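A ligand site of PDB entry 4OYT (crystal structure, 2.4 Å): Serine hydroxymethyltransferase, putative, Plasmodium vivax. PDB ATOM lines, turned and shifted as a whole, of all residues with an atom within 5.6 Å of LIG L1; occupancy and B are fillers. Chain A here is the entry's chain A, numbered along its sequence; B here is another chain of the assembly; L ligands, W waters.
The side-chain hydroxyl (OG) of Ser 100 is in hydrogen-bond range of an oxygen (O4) of LIG L1 (2.5 Å). The side-chain hydroxyl of Tyr 54 of chain B sits at hydrogen-bond distance from an oxygen (O6) of LIG L1. O1 of LIG L1 sits at hydrogen-bond distance from NE2 of His 211. OG of Ser 34 lies within hydrogen-bond range of O8 of LIG L1 (2.6 Å). OE1 of Glu 56 of chain B sits at hydrogen-bond distance from O3 of LIG L1 (2.6 Å). O5 of LIG L1 is in hydrogen-bond range of N of Ser 102, at 2.9 Å. The side-chain hydroxyl of Ser 102 lies within hydrogen-bond range of an oxygen (O5) of LIG L1 (2.7 Å). The side-chain hydroxyl (OH) of Tyr 64 of chain B lies within hydrogen-bond range of an oxygen (O8) of LIG L1 (2.7 Å). OD2 of Asp 208 sits at hydrogen-bond distance from N2 of LIG L1, at 2.7 Å. O8 of LIG L1 is in salt-bridge range of NH2 of Arg 371, at 2.9 Å. N of Gly 101 is in hydrogen-bond range of O4 of LIG L1. OG1 of Thr 183 is in hydrogen-bond range of O2 of LIG L1 (3.0 Å). A ring nitrogen (NE2) of His 236 lies close to an oxygen (O4) of LIG L1 (3.3 Å). The backbone NH (N) of Gly 272 of chain B lies within hydrogen-bond range of an oxygen (O6) of LIG L1 (3.3 Å). ND1 of His 129 lies within hydrogen-bond range of O1 of LG2 L2.
The side-chain hydroxyl of Ser 100 sits at hydrogen-bond distance from a ring nitrogen (NE2) of His 274 of chain B, at 3.2 Å. The side-chain hydroxyl (OH) of Tyr 54 of chain B sits at hydrogen-bond distance from a ring nitrogen (NE2) of His 236 (3.2 Å). The side-chain hydroxyl of Tyr 54 of chain B sits at hydrogen-bond distance from the side-chain amino group of Lys 237. The side-chain hydroxyl of Ser 102 is in hydrogen-bond range of a ring nitrogen (NE2) of His 129 (3.2 Å). The side-chain hydroxyl (OG) of Ser 102 lies within hydrogen-bond range of the backbone NH (N) of Gly 271 of chain B, at 3.5 Å. NH2 of Arg 371 lies within hydrogen-bond range of OH of Tyr 64 of chain B (3.2 Å). The guanidinium group (NH1) of Arg 371 lies within hydrogen-bond range of the backbone carbonyl oxygen (O) of Thr 183. The side-chain hydroxyl (OG1) of Thr 183 lies close to a ring nitrogen (ND1) of His 129.
Residues that only touch LIG L1: His 129, Lys 237, Thr 234, Tyr 182, Gly 271 of chain B, Asn 105 and Ser 210. The nearest printed residue that does not touch LIG L1 is His 132 (4.3 Å).
Water W1 lies within hydrogen-bond range of N of Gly 271 of chain B (2.6 Å), O5 of LIG L1 (2.7 Å) and OG of Ser 100 (3.2 Å). Water W2 lies within hydrogen-bond range of NH2 of Arg 243 (2.6 Å), O6 of LIG L1 (2.9 Å), O of Gly 272 of chain B (3.1 Å) and OG of Ser 100 (3.4 Å).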
ATOM      1  N   ILE A  32      17.725 -29.082 -29.511  1.00  0.00           N
ATOM      2  CA  ILE A  32      17.223 -28.607 -28.232  1.00  0.00           C
ATOM      3  C   ILE A  32      17.512 -29.688 -27.190  1.00  0.00           C
ATOM      4  O   ILE A  32      17.095 -30.833 -27.332  1.00  0.00           O
ATOM      5  CB  ILE A  32      15.744 -28.202 -28.325  1.00  0.00           C
ATOM      6  CG1 ILE A  32      15.669 -26.826 -29.022  1.00  0.00           C
ATOM      7  CG2 ILE A  32      15.123 -28.156 -26.950  1.00  0.00           C
ATOM      8  CD1 ILE A  32      14.316 -26.459 -29.588  1.00  0.00           C
ATOM      9  N   SER A  34      16.747 -30.514 -24.267  1.00  0.00           N
ATOM     10  CA  SER A  34      15.729 -31.125 -23.436  1.00  0.00           C
ATOM     11  C   SER A  34      14.627 -31.848 -24.233  1.00  0.00           C
ATOM     12  O   SER A  34      13.626 -32.268 -23.655  1.00  0.00           O
ATOM     13  CB  SER A  34      15.122 -30.065 -22.533  1.00  0.00           C
ATOM     14  OG  SER A  34      14.679 -28.990 -23.321  1.00  0.00           O
ATOM     15  N   SER A 100       4.603 -32.703 -13.868  1.00  0.00           N
ATOM     16  CA  SER A 100       5.733 -32.177 -14.608  1.00  0.00           C
ATOM     17  C   SER A 100       6.922 -31.941 -13.677  1.00  0.00           C
ATOM     18  O   SER A 100       6.791 -32.007 -12.459  1.00  0.00           O
ATOM     19  CB  SER A 100       5.341 -30.873 -15.293  1.00  0.00           C
ATOM     20  OG  SER A 100       5.888 -30.813 -16.613  1.00  0.00           O
ATOM     21  N   GLY A 101       8.085 -31.642 -14.251  1.00  0.00           N
ATOM     22  CA  GLY A 101       9.294 -31.468 -13.475  1.00  0.00           C
ATOM     23  C   GLY A 101       9.223 -30.324 -12.508  1.00  0.00           C
ATOM     24  O   GLY A 101       9.715 -30.416 -11.396  1.00  0.00           O
ATOM     25  N   SER A 102       8.606 -29.234 -12.966  1.00  0.00           N
ATOM     26  CA  SER A 102       8.389 -28.036 -12.171  1.00  0.00           C
ATOM     27  C   SER A 102       7.444 -28.285 -10.998  1.00  0.00           C
ATOM     28  O   SER A 102       7.626 -27.722  -9.930  1.00  0.00           O
ATOM     29  CB  SER A 102       7.865 -26.922 -13.072  1.00  0.00           C
ATOM     30  OG  SER A 102       8.822 -26.592 -14.084  1.00  0.00           O
ATOM     31  N   ALA A 103       6.435 -29.129 -11.206  1.00  0.00           N
ATOM     32  CA  ALA A 103       5.532 -29.540 -10.112  1.00  0.00           C
ATOM     33  C   ALA A 103       6.258 -30.436  -9.084  1.00  0.00           C
ATOM     34  O   ALA A 103       6.137 -30.219  -7.885  1.00  0.00           O
ATOM     35  CB  ALA A 103       4.317 -30.266 -10.685  1.00  0.00           C
ATOM     36  N   ASN A 105       9.504 -30.595  -8.366  1.00  0.00           N
ATOM     37  CA  ASN A 105      10.358 -29.734  -7.564  1.00  0.00           C
ATOM     38  C   ASN A 105       9.628 -28.876  -6.532  1.00  0.00           C
ATOM     39  O   ASN A 105      10.030 -28.837  -5.369  1.00  0.00           O
ATOM     40  CB  ASN A 105      11.279 -28.886  -8.435  1.00  0.00           C
ATOM     41  CG  ASN A 105      12.262 -29.720  -9.201  1.00  0.00           C
ATOM     42  OD1 ASN A 105      12.523 -30.877  -8.842  1.00  0.00           O
ATOM     43  ND2 ASN A 105      12.852 -29.145 -10.251  1.00  0.00           N
ATOM     44  N   HIS A 129      17.520 -24.313 -12.956  1.00  0.00           N
ATOM     45  CA  HIS A 129      16.147 -24.216 -13.434  1.00  0.00           C
ATOM     46  C   HIS A 129      15.378 -23.205 -12.647  1.00  0.00           C
ATOM     47  O   HIS A 129      15.779 -22.844 -11.517  1.00  0.00           O
ATOM     48  CB  HIS A 129      15.450 -25.575 -13.348  1.00  0.00           C
ATOM     49  CG  HIS A 129      14.050 -25.571 -13.915  1.00  0.00           C
ATOM     50  ND1 HIS A 129      13.799 -25.513 -15.241  1.00  0.00           N
ATOM     51  CD2 HIS A 129      12.813 -25.623 -13.281  1.00  0.00           C
ATOM     52  CE1 HIS A 129      12.468 -25.501 -15.434  1.00  0.00           C
ATOM     53  NE2 HIS A 129      11.867 -25.572 -14.237  1.00  0.00           N
ATOM     54  N   THR A 131      12.586 -23.509 -11.011  1.00  0.00           N
ATOM     55  CA  THR A 131      12.136 -24.034  -9.729  1.00  0.00           C
ATOM     56  C   THR A 131      13.298 -24.328  -8.764  1.00  0.00           C
ATOM     57  O   THR A 131      13.132 -25.067  -7.807  1.00  0.00           O
ATOM     58  CB  THR A 131      11.296 -25.307  -9.908  1.00  0.00           C
ATOM     59  OG1 THR A 131      12.075 -26.297 -10.596  1.00  0.00           O
ATOM     60  CG2 THR A 131      10.023 -24.975 -10.714  1.00  0.00           C
ATOM     61  N   HIS A 132      14.479 -23.750  -9.009  1.00  0.00           N
ATOM     62  CA  HIS A 132      15.575 -23.875  -8.057  1.00  0.00           C
ATOM     63  C   HIS A 132      15.728 -22.591  -7.302  1.00  0.00           C
ATOM     64  O   HIS A 132      16.792 -22.304  -6.754  1.00  0.00           O
ATOM     65  CB  HIS A 132      16.881 -24.302  -8.723  1.00  0.00           C
ATOM     66  CG  HIS A 132      16.812 -25.643  -9.422  1.00  0.00           C
ATOM     67  ND1 HIS A 132      17.806 -26.090 -10.220  1.00  0.00           N
ATOM     68  CD2 HIS A 132      15.825 -26.623  -9.453  1.00  0.00           C
ATOM     69  CE1 HIS A 132      17.481 -27.310 -10.706  1.00  0.00           C
ATOM     70  NE2 HIS A 132      16.258 -27.624 -10.243  1.00  0.00           N
ATOM     71  N   GLY A 181      22.159 -30.210  -9.774  1.00  0.00           N
ATOM     72  CA  GLY A 181      21.580 -30.852 -10.964  1.00  0.00           C
ATOM     73  C   GLY A 181      20.833 -29.760 -11.718  1.00  0.00           C
ATOM     74  O   GLY A 181      20.040 -29.032 -11.130  1.00  0.00           O
ATOM     75  N   TYR A 182      21.098 -29.636 -13.016  1.00  0.00           N
ATOM     76  CA  TYR A 182      20.860 -28.364 -13.676  1.00  0.00           C
ATOM     77  C   TYR A 182      20.188 -28.466 -15.020  1.00  0.00           C
ATOM     78  O   TYR A 182      19.969 -29.568 -15.547  1.00  0.00           O
ATOM     79  CB  TYR A 182      22.174 -27.575 -13.755  1.00  0.00           C
ATOM     80  CG  TYR A 182      22.967 -27.585 -12.454  1.00  0.00           C
ATOM     81  CD1 TYR A 182      22.506 -26.901 -11.323  1.00  0.00           C
ATOM     82  CD2 TYR A 182      24.158 -28.303 -12.352  1.00  0.00           C
ATOM     83  CE1 TYR A 182      23.228 -26.924 -10.139  1.00  0.00           C
ATOM     84  CE2 TYR A 182      24.889 -28.325 -11.171  1.00  0.00           C
ATOM     85  CZ  TYR A 182      24.417 -27.630 -10.065  1.00  0.00           C
ATOM     86  OH  TYR A 182      25.148 -27.670  -8.893  1.00  0.00           O
ATOM     87  N   THR A 183      19.830 -27.305 -15.559  1.00  0.00           N
ATOM     88  CA  THR A 183      19.137 -27.187 -16.831  1.00  0.00           C
ATOM     89  C   THR A 183      20.139 -27.028 -17.975  1.00  0.00           C
ATOM     90  O   THR A 183      19.974 -27.615 -19.038  1.00  0.00           O
ATOM     91  CB  THR A 183      18.178 -25.996 -16.812  1.00  0.00           C
ATOM     92  OG1 THR A 183      17.118 -26.286 -15.890  1.00  0.00           O
ATOM     93  CG2 THR A 183      17.592 -25.711 -18.186  1.00  0.00           C
ATOM     94  N   ASP A 208      18.378 -32.555  -8.879  1.00  0.00           N
ATOM     95  CA  ASP A 208      17.456 -32.575 -10.042  1.00  0.00           C
ATOM     96  C   ASP A 208      18.258 -33.015 -11.248  1.00  0.00           C
ATOM     97  O   ASP A 208      19.045 -32.227 -11.770  1.00  0.00           O
ATOM     98  CB  ASP A 208      16.884 -31.175 -10.287  1.00  0.00           C
ATOM     99  CG  ASP A 208      15.858 -31.127 -11.409  1.00  0.00           C
ATOM    100  OD1 ASP A 208      15.749 -32.091 -12.193  1.00  0.00           O
ATOM    101  OD2 ASP A 208      15.161 -30.078 -11.509  1.00  0.00           O
ATOM    102  N   SER A 210      16.999 -34.228 -14.201  1.00  0.00           N
ATOM    103  CA  SER A 210      16.156 -34.248 -15.386  1.00  0.00           C
ATOM    104  C   SER A 210      16.922 -34.246 -16.721  1.00  0.00           C
ATOM    105  O   SER A 210      16.504 -34.912 -17.685  1.00  0.00           O
ATOM    106  CB  SER A 210      15.181 -33.073 -15.332  1.00  0.00           C
ATOM    107  OG  SER A 210      14.243 -33.227 -14.273  1.00  0.00           O
ATOM    108  N   HIS A 211      18.035 -33.510 -16.783  1.00  0.00           N
ATOM    109  CA  HIS A 211      18.831 -33.474 -18.022  1.00  0.00           C
ATOM    110  C   HIS A 211      19.760 -34.627 -18.223  1.00  0.00           C
ATOM    111  O   HIS A 211      20.115 -34.966 -19.367  1.00  0.00           O
ATOM    112  CB  HIS A 211      19.581 -32.165 -18.165  1.00  0.00           C
ATOM    113  CG  HIS A 211      18.844 -31.151 -19.017  1.00  0.00           C
ATOM    114  ND1 HIS A 211      19.188 -30.881 -20.296  1.00  0.00           N
ATOM    115  CD2 HIS A 211      17.727 -30.374 -18.737  1.00  0.00           C
ATOM    116  CE1 HIS A 211      18.348 -29.961 -20.792  1.00  0.00           C
ATOM    117  NE2 HIS A 211      17.446 -29.651 -19.836  1.00  0.00           N
ATOM    118  N   THR A 234      12.509 -35.365 -14.590  1.00  0.00           N
ATOM    119  CA  THR A 234      11.432 -35.396 -15.561  1.00  0.00           C
ATOM    120  C   THR A 234      11.575 -36.723 -16.263  1.00  0.00           C
ATOM    121  O   THR A 234      12.645 -37.314 -16.228  1.00  0.00           O
ATOM    122  CB  THR A 234      11.544 -34.250 -16.595  1.00  0.00           C
ATOM    123  OG1 THR A 234      12.872 -34.236 -17.144  1.00  0.00           O
ATOM    124  CG2 THR A 234      11.232 -32.903 -15.963  1.00  0.00           C
ATOM    125  N   HIS A 236      10.763 -37.052 -19.593  1.00  0.00           N
ATOM    126  CA  HIS A 236      10.591 -36.755 -21.036  1.00  0.00           C
ATOM    127  C   HIS A 236      11.778 -36.204 -21.755  1.00  0.00           C
ATOM    128  O   HIS A 236      11.677 -35.892 -22.963  1.00  0.00           O
ATOM    129  CB  HIS A 236       9.417 -35.808 -21.280  1.00  0.00           C
ATOM    130  CG  HIS A 236       9.404 -34.596 -20.391  1.00  0.00           C
ATOM    131  ND1 HIS A 236       8.861 -34.607 -19.156  1.00  0.00           N
ATOM    132  CD2 HIS A 236       9.876 -33.305 -20.597  1.00  0.00           C
ATOM    133  CE1 HIS A 236       8.983 -33.385 -18.605  1.00  0.00           C
ATOM    134  NE2 HIS A 236       9.611 -32.593 -19.479  1.00  0.00           N
ATOM    135  N   LYS A 237      12.909 -36.068 -21.091  1.00  0.00           N
ATOM    136  CA  LYS A 237      14.033 -35.510 -21.803  1.00  0.00           C
ATOM    137  C   LYS A 237      14.887 -36.662 -22.301  1.00  0.00           C
ATOM    138  O   LYS A 237      14.413 -37.521 -23.032  1.00  0.00           O
ATOM    139  CB  LYS A 237      14.814 -34.524 -20.937  1.00  0.00           C
ATOM    140  CG  LYS A 237      14.004 -33.324 -20.472  1.00  0.00           C
ATOM    141  CD  LYS A 237      14.892 -32.447 -19.630  1.00  0.00           C
ATOM    142  CE  LYS A 237      14.164 -31.237 -19.113  1.00  0.00           C
ATOM    143  NZ  LYS A 237      12.771 -31.628 -18.799  1.00  0.00           N
ATOM    144  N   ARG A 243       5.609 -36.676 -20.844  1.00  0.00           N
ATOM    145  CA  ARG A 243       5.847 -35.507 -20.025  1.00  0.00           C
ATOM    146  C   ARG A 243       5.280 -35.751 -18.637  1.00  0.00           C
ATOM    147  O   ARG A 243       4.054 -35.802 -18.420  1.00  0.00           O
ATOM    148  CB  ARG A 243       5.253 -34.238 -20.661  1.00  0.00           C
ATOM    149  CG  ARG A 243       5.574 -34.047 -22.130  1.00  0.00           C
ATOM    150  CD  ARG A 243       5.203 -32.628 -22.584  1.00  0.00           C
ATOM    151  NE  ARG A 243       6.142 -31.633 -22.053  1.00  0.00           N
ATOM    152  CZ  ARG A 243       7.274 -31.286 -22.663  1.00  0.00           C
ATOM    153  NH1 ARG A 243       7.632 -31.842 -23.810  1.00  0.00           N
ATOM    154  NH2 ARG A 243       8.049 -30.377 -22.088  1.00  0.00           N
ATOM    155  N   SER A 244       6.178 -35.920 -17.689  1.00  0.00           N
ATOM    156  CA  SER A 244       5.818 -36.237 -16.330  1.00  0.00           C
ATOM    157  C   SER A 244       7.069 -36.141 -15.501  1.00  0.00           C
ATOM    158  O   SER A 244       8.122 -35.761 -16.014  1.00  0.00           O
ATOM    159  CB  SER A 244       5.241 -37.662 -16.267  1.00  0.00           C
ATOM    160  OG  SER A 244       4.658 -37.855 -14.991  1.00  0.00           O
ATOM    161  N   ASN A 354      18.610 -23.245 -28.774  1.00  0.00           N
ATOM    162  CA  ASN A 354      18.126 -22.116 -27.976  1.00  0.00           C
ATOM    163  C   ASN A 354      19.275 -21.275 -27.441  1.00  0.00           C
ATOM    164  O   ASN A 354      20.344 -21.798 -27.139  1.00  0.00           O
ATOM    165  CB  ASN A 354      17.145 -22.562 -26.876  1.00  0.00           C
ATOM    166  CG  ASN A 354      17.771 -23.512 -25.852  1.00  0.00           C
ATOM    167  OD1 ASN A 354      17.819 -24.718 -26.046  1.00  0.00           O
ATOM    168  ND2 ASN A 354      18.270 -22.944 -24.743  1.00  0.00           N
ATOM    169  N   ARG A 371      22.761 -23.306 -26.604  1.00  0.00           N
ATOM    170  CA  ARG A 371      22.879 -24.641 -26.096  1.00  0.00           C
ATOM    171  C   ARG A 371      22.436 -25.626 -27.156  1.00  0.00           C
ATOM    172  O   ARG A 371      21.381 -25.467 -27.769  1.00  0.00           O
ATOM    173  CB  ARG A 371      22.028 -24.782 -24.821  1.00  0.00           C
ATOM    174  CG  ARG A 371      21.934 -26.207 -24.285  1.00  0.00           C
ATOM    175  CD  ARG A 371      20.971 -26.245 -23.093  1.00  0.00           C
ATOM    176  NE  ARG A 371      19.586 -26.205 -23.544  1.00  0.00           N
ATOM    177  CZ  ARG A 371      18.547 -26.402 -22.755  1.00  0.00           C
ATOM    178  NH1 ARG A 371      18.736 -26.666 -21.458  1.00  0.00           N
ATOM    179  NH2 ARG A 371      17.323 -26.348 -23.258  1.00  0.00           N
ATOM    180  N   TYR B  54       8.878 -28.582 -26.799  1.00  0.00           N
ATOM    181  CA  TYR B  54       8.940 -27.618 -25.699  1.00  0.00           C
ATOM    182  C   TYR B  54       8.469 -26.244 -26.153  1.00  0.00           C
ATOM    183  O   TYR B  54       8.962 -25.694 -27.124  1.00  0.00           O
ATOM    184  CB  TYR B  54      10.343 -27.553 -25.091  1.00  0.00           C
ATOM    185  CG  TYR B  54      10.429 -28.101 -23.676  1.00  0.00           C
ATOM    186  CD1 TYR B  54       9.781 -27.447 -22.630  1.00  0.00           C
ATOM    187  CD2 TYR B  54      11.174 -29.262 -23.376  1.00  0.00           C
ATOM    188  CE1 TYR B  54       9.841 -27.937 -21.319  1.00  0.00           C
ATOM    189  CE2 TYR B  54      11.247 -29.755 -22.060  1.00  0.00           C
ATOM    190  CZ  TYR B  54      10.570 -29.092 -21.033  1.00  0.00           C
ATOM    191  OH  TYR B  54      10.609 -29.545 -19.732  1.00  0.00           O
ATOM    192  N   GLU B  56       7.624 -23.491 -23.776  1.00  0.00           N
ATOM    193  CA  GLU B  56       7.556 -22.527 -22.679  1.00  0.00           C
ATOM    194  C   GLU B  56       7.371 -21.089 -23.147  1.00  0.00           C
ATOM    195  O   GLU B  56       8.076 -20.606 -24.040  1.00  0.00           O
ATOM    196  CB  GLU B  56       8.771 -22.649 -21.755  1.00  0.00           C
ATOM    197  CG  GLU B  56      10.099 -22.896 -22.456  1.00  0.00           C
ATOM    198  CD  GLU B  56      11.074 -23.633 -21.559  1.00  0.00           C
ATOM    199  OE1 GLU B  56      10.699 -23.878 -20.386  1.00  0.00           O
ATOM    200  OE2 GLU B  56      12.201 -23.965 -22.023  1.00  0.00           O
ATOM    201  N   TYR B  64      11.722 -20.528 -27.234  1.00  0.00           N
ATOM    202  CA  TYR B  64      12.343 -21.239 -28.352  1.00  0.00           C
ATOM    203  C   TYR B  64      11.568 -20.976 -29.630  1.00  0.00           C
ATOM    204  O   TYR B  64      10.448 -20.488 -29.584  1.00  0.00           O
ATOM    205  CB  TYR B  64      12.377 -22.746 -28.097  1.00  0.00           C
ATOM    206  CG  TYR B  64      13.008 -23.169 -26.781  1.00  0.00           C
ATOM    207  CD1 TYR B  64      13.802 -22.277 -26.045  1.00  0.00           C
ATOM    208  CD2 TYR B  64      12.842 -24.462 -26.297  1.00  0.00           C
ATOM    209  CE1 TYR B  64      14.391 -22.664 -24.860  1.00  0.00           C
ATOM    210  CE2 TYR B  64      13.431 -24.858 -25.115  1.00  0.00           C
ATOM    211  CZ  TYR B  64      14.204 -23.948 -24.397  1.00  0.00           C
ATOM    212  OH  TYR B  64      14.794 -24.325 -23.208  1.00  0.00           O
ATOM    213  N   GLN B 270       4.397 -23.485 -13.620  1.00  0.00           N
ATOM    214  CA  GLN B 270       4.690 -24.500 -14.625  1.00  0.00           C
ATOM    215  C   GLN B 270       5.925 -24.170 -15.464  1.00  0.00           C
ATOM    216  O   GLN B 270       6.443 -23.058 -15.417  1.00  0.00           O
ATOM    217  CB  GLN B 270       3.469 -24.746 -15.559  1.00  0.00           C
ATOM    218  CG  GLN B 270       2.159 -25.014 -14.812  1.00  0.00           C
ATOM    219  CD  GLN B 270       1.066 -25.677 -15.646  1.00  0.00           C
ATOM    220  OE1 GLN B 270       0.102 -26.204 -15.072  1.00  0.00           O
ATOM    221  NE2 GLN B 270       1.201 -25.652 -16.990  1.00  0.00           N
ATOM    222  N   GLY B 271       6.423 -25.177 -16.167  1.00  0.00           N
ATOM    223  CA  GLY B 271       7.381 -24.975 -17.237  1.00  0.00           C
ATOM    224  C   GLY B 271       6.668 -25.165 -18.555  1.00  0.00           C
ATOM    225  O   GLY B 271       5.634 -24.544 -18.805  1.00  0.00           O
ATOM    226  N   GLY B 272       7.205 -26.027 -19.410  1.00  0.00           N
ATOM    227  CA  GLY B 272       6.652 -26.195 -20.753  1.00  0.00           C
ATOM    228  C   GLY B 272       5.244 -26.724 -20.694  1.00  0.00           C
ATOM    229  O   GLY B 272       4.946 -27.582 -19.863  1.00  0.00           O
ATOM    230  N   HIS B 274       1.909 -28.882 -21.819  1.00  0.00           N
ATOM    231  CA  HIS B 274       1.697 -30.179 -22.448  1.00  0.00           C
ATOM    232  C   HIS B 274       0.826 -29.996 -23.672  1.00  0.00           C
ATOM    233  O   HIS B 274      -0.403 -29.840 -23.574  1.00  0.00           O
ATOM    234  CB  HIS B 274       1.103 -31.177 -21.456  1.00  0.00           C
ATOM    235  CG  HIS B 274       2.032 -31.537 -20.301  1.00  0.00           C
ATOM    236  ND1 HIS B 274       1.898 -32.668 -19.592  1.00  0.00           N
ATOM    237  CD2 HIS B 274       3.126 -30.855 -19.754  1.00  0.00           C
ATOM    238  CE1 HIS B 274       2.837 -32.715 -18.620  1.00  0.00           C
ATOM    239  NE2 HIS B 274       3.588 -31.606 -18.735  1.00  0.00           N
HETATM  240  C1  LIG L   1      14.851 -27.167 -20.766  1.00  0.00           C
HETATM  241  N1  LIG L   1      13.919 -27.212 -18.387  1.00  0.00           N
HETATM  242  O1  LIG L   1      15.920 -27.722 -20.419  1.00  0.00           O
HETATM  243  P1  LIG L   1       8.796 -29.328 -16.899  1.00  0.00           P
HETATM  244  N2  LIG L   1      14.054 -29.337 -13.902  1.00  0.00           N
HETATM  245  C2  LIG L   1      15.025 -29.257 -14.726  1.00  0.00           C
HETATM  246  C3  LIG L   1      14.800 -28.913 -16.054  1.00  0.00           C
HETATM  247  O2  LIG L   1      15.876 -28.841 -16.856  1.00  0.00           O
HETATM  248  C4  LIG L   1      13.530 -28.635 -16.519  1.00  0.00           C
HETATM  249  C5  LIG L   1      12.513 -28.759 -15.577  1.00  0.00           C
HETATM  250  C6  LIG L   1      12.861 -29.113 -14.272  1.00  0.00           C
HETATM  251  C7  LIG L   1      13.955 -26.551 -19.710  1.00  0.00           C
HETATM  252  C8  LIG L   1      12.534 -26.476 -20.213  1.00  0.00           C
HETATM  253  O3  LIG L   1      11.644 -26.041 -19.194  1.00  0.00           O
HETATM  254  O4  LIG L   1       8.330 -30.764 -17.102  1.00  0.00           O
HETATM  255  C9  LIG L   1      16.443 -29.541 -14.268  1.00  0.00           C
HETATM  256  O5  LIG L   1       8.099 -28.600 -15.774  1.00  0.00           O
HETATM  257  O6  LIG L   1       8.948 -28.528 -18.164  1.00  0.00           O
HETATM  258  C10 LIG L   1      13.321 -28.250 -17.965  1.00  0.00           C
HETATM  259  O7  LIG L   1      10.324 -29.557 -16.441  1.00  0.00           O
HETATM  260  C11 LIG L   1      11.050 -28.476 -15.862  1.00  0.00           C
HETATM  261  O8  LIG L   1      14.720 -26.755 -21.951  1.00  0.00           O
HETATM  262  N1  LG2 L   2      17.676 -22.344 -19.064  1.00  0.00           N
HETATM  263  C1  LG2 L   2      17.898 -22.534 -17.760  1.00  0.00           C
HETATM  264  N2  LG2 L   2      19.181 -22.660 -17.339  1.00  0.00           N
HETATM  265  N3  LG2 L   2      16.902 -22.636 -16.841  1.00  0.00           N
HETATM  266  C2  LG2 L   2      15.584 -22.532 -17.163  1.00  0.00           C
HETATM  267  O1  LG2 L   2      14.677 -22.615 -16.286  1.00  0.00           O
HETATM  268  C3  LG2 L   2      15.305 -22.340 -18.594  1.00  0.00           C
HETATM  269  N4  LG2 L   2      14.069 -22.148 -19.184  1.00  0.00           N
HETATM  270  C4  LG2 L   2      14.216 -20.986 -20.085  1.00  0.00           C
HETATM  271  C5  LG2 L   2      14.883 -21.549 -21.334  1.00  0.00           C
HETATM  272  N5  LG2 L   2      16.187 -22.035 -20.870  1.00  0.00           N
HETATM  273  C6  LG2 L   2      16.443 -22.227 -19.535  1.00  0.00           C
HETATM  274  C7  LG2 L   2      12.946 -20.178 -20.242  1.00  0.00           C
HETATM  275  N6  LG2 L   2      12.736 -19.688 -18.895  1.00  0.00           N
HETATM  276  C8  LG2 L   2      12.900 -15.846 -17.391  1.00  0.00           C
HETATM  277  C9  LG2 L   2      14.003 -16.336 -18.114  1.00  0.00           C
HETATM  278  C10 LG2 L   2      13.989 -17.625 -18.637  1.00  0.00           C
HETATM  279  C11 LG2 L   2      12.855 -18.419 -18.450  1.00  0.00           C
HETATM  280  C12 LG2 L   2      11.775 -17.929 -17.725  1.00  0.00           C
HETATM  281  C13 LG2 L   2      11.789 -16.640 -17.202  1.00  0.00           C
HETATM  282  C14 LG2 L   2      12.871 -14.468 -16.798  1.00  0.00           C
HETATM  283  O2  LG2 L   2      13.907 -13.838 -16.673  1.00  0.00           O
HETATM  284  N7  LG2 L   2      11.670 -14.000 -16.418  1.00  0.00           N
HETATM  285  C15 LG2 L   2      11.260 -12.604 -16.335  1.00  0.00           C
HETATM  286  C16 LG2 L   2      11.343 -11.907 -17.687  1.00  0.00           C
HETATM  287  C17 LG2 L   2      11.860 -10.473 -17.554  1.00  0.00           C
HETATM  288  C18 LG2 L   2      12.563 -10.036 -18.832  1.00  0.00           C
HETATM  289  O3  LG2 L   2      12.401 -10.731 -19.874  1.00  0.00           O
HETATM  290  O4  LG2 L   2      13.277  -9.008 -18.790  1.00  0.00           O
HETATM  291  C19 LG2 L   2       9.853 -12.491 -15.824  1.00  0.00           C
HETATM  292  O5  LG2 L   2       9.040 -13.416 -16.095  1.00  0.00           O
HETATM  293  O6  LG2 L   2       9.532 -11.485 -15.141  1.00  0.00           O
HETATM  294  C20 LG2 L   2      13.062 -22.911 -18.991  1.00  0.00           C
HETATM  295  O7  LG2 L   2      12.061 -22.586 -18.363  1.00  0.00           O
HETATM  296  O   HOH W   1       5.668 -27.666 -16.349  1.00  0.00           O
HETATM  297  O   HOH W   2       6.983 -29.960 -19.715  1.00  0.00           O
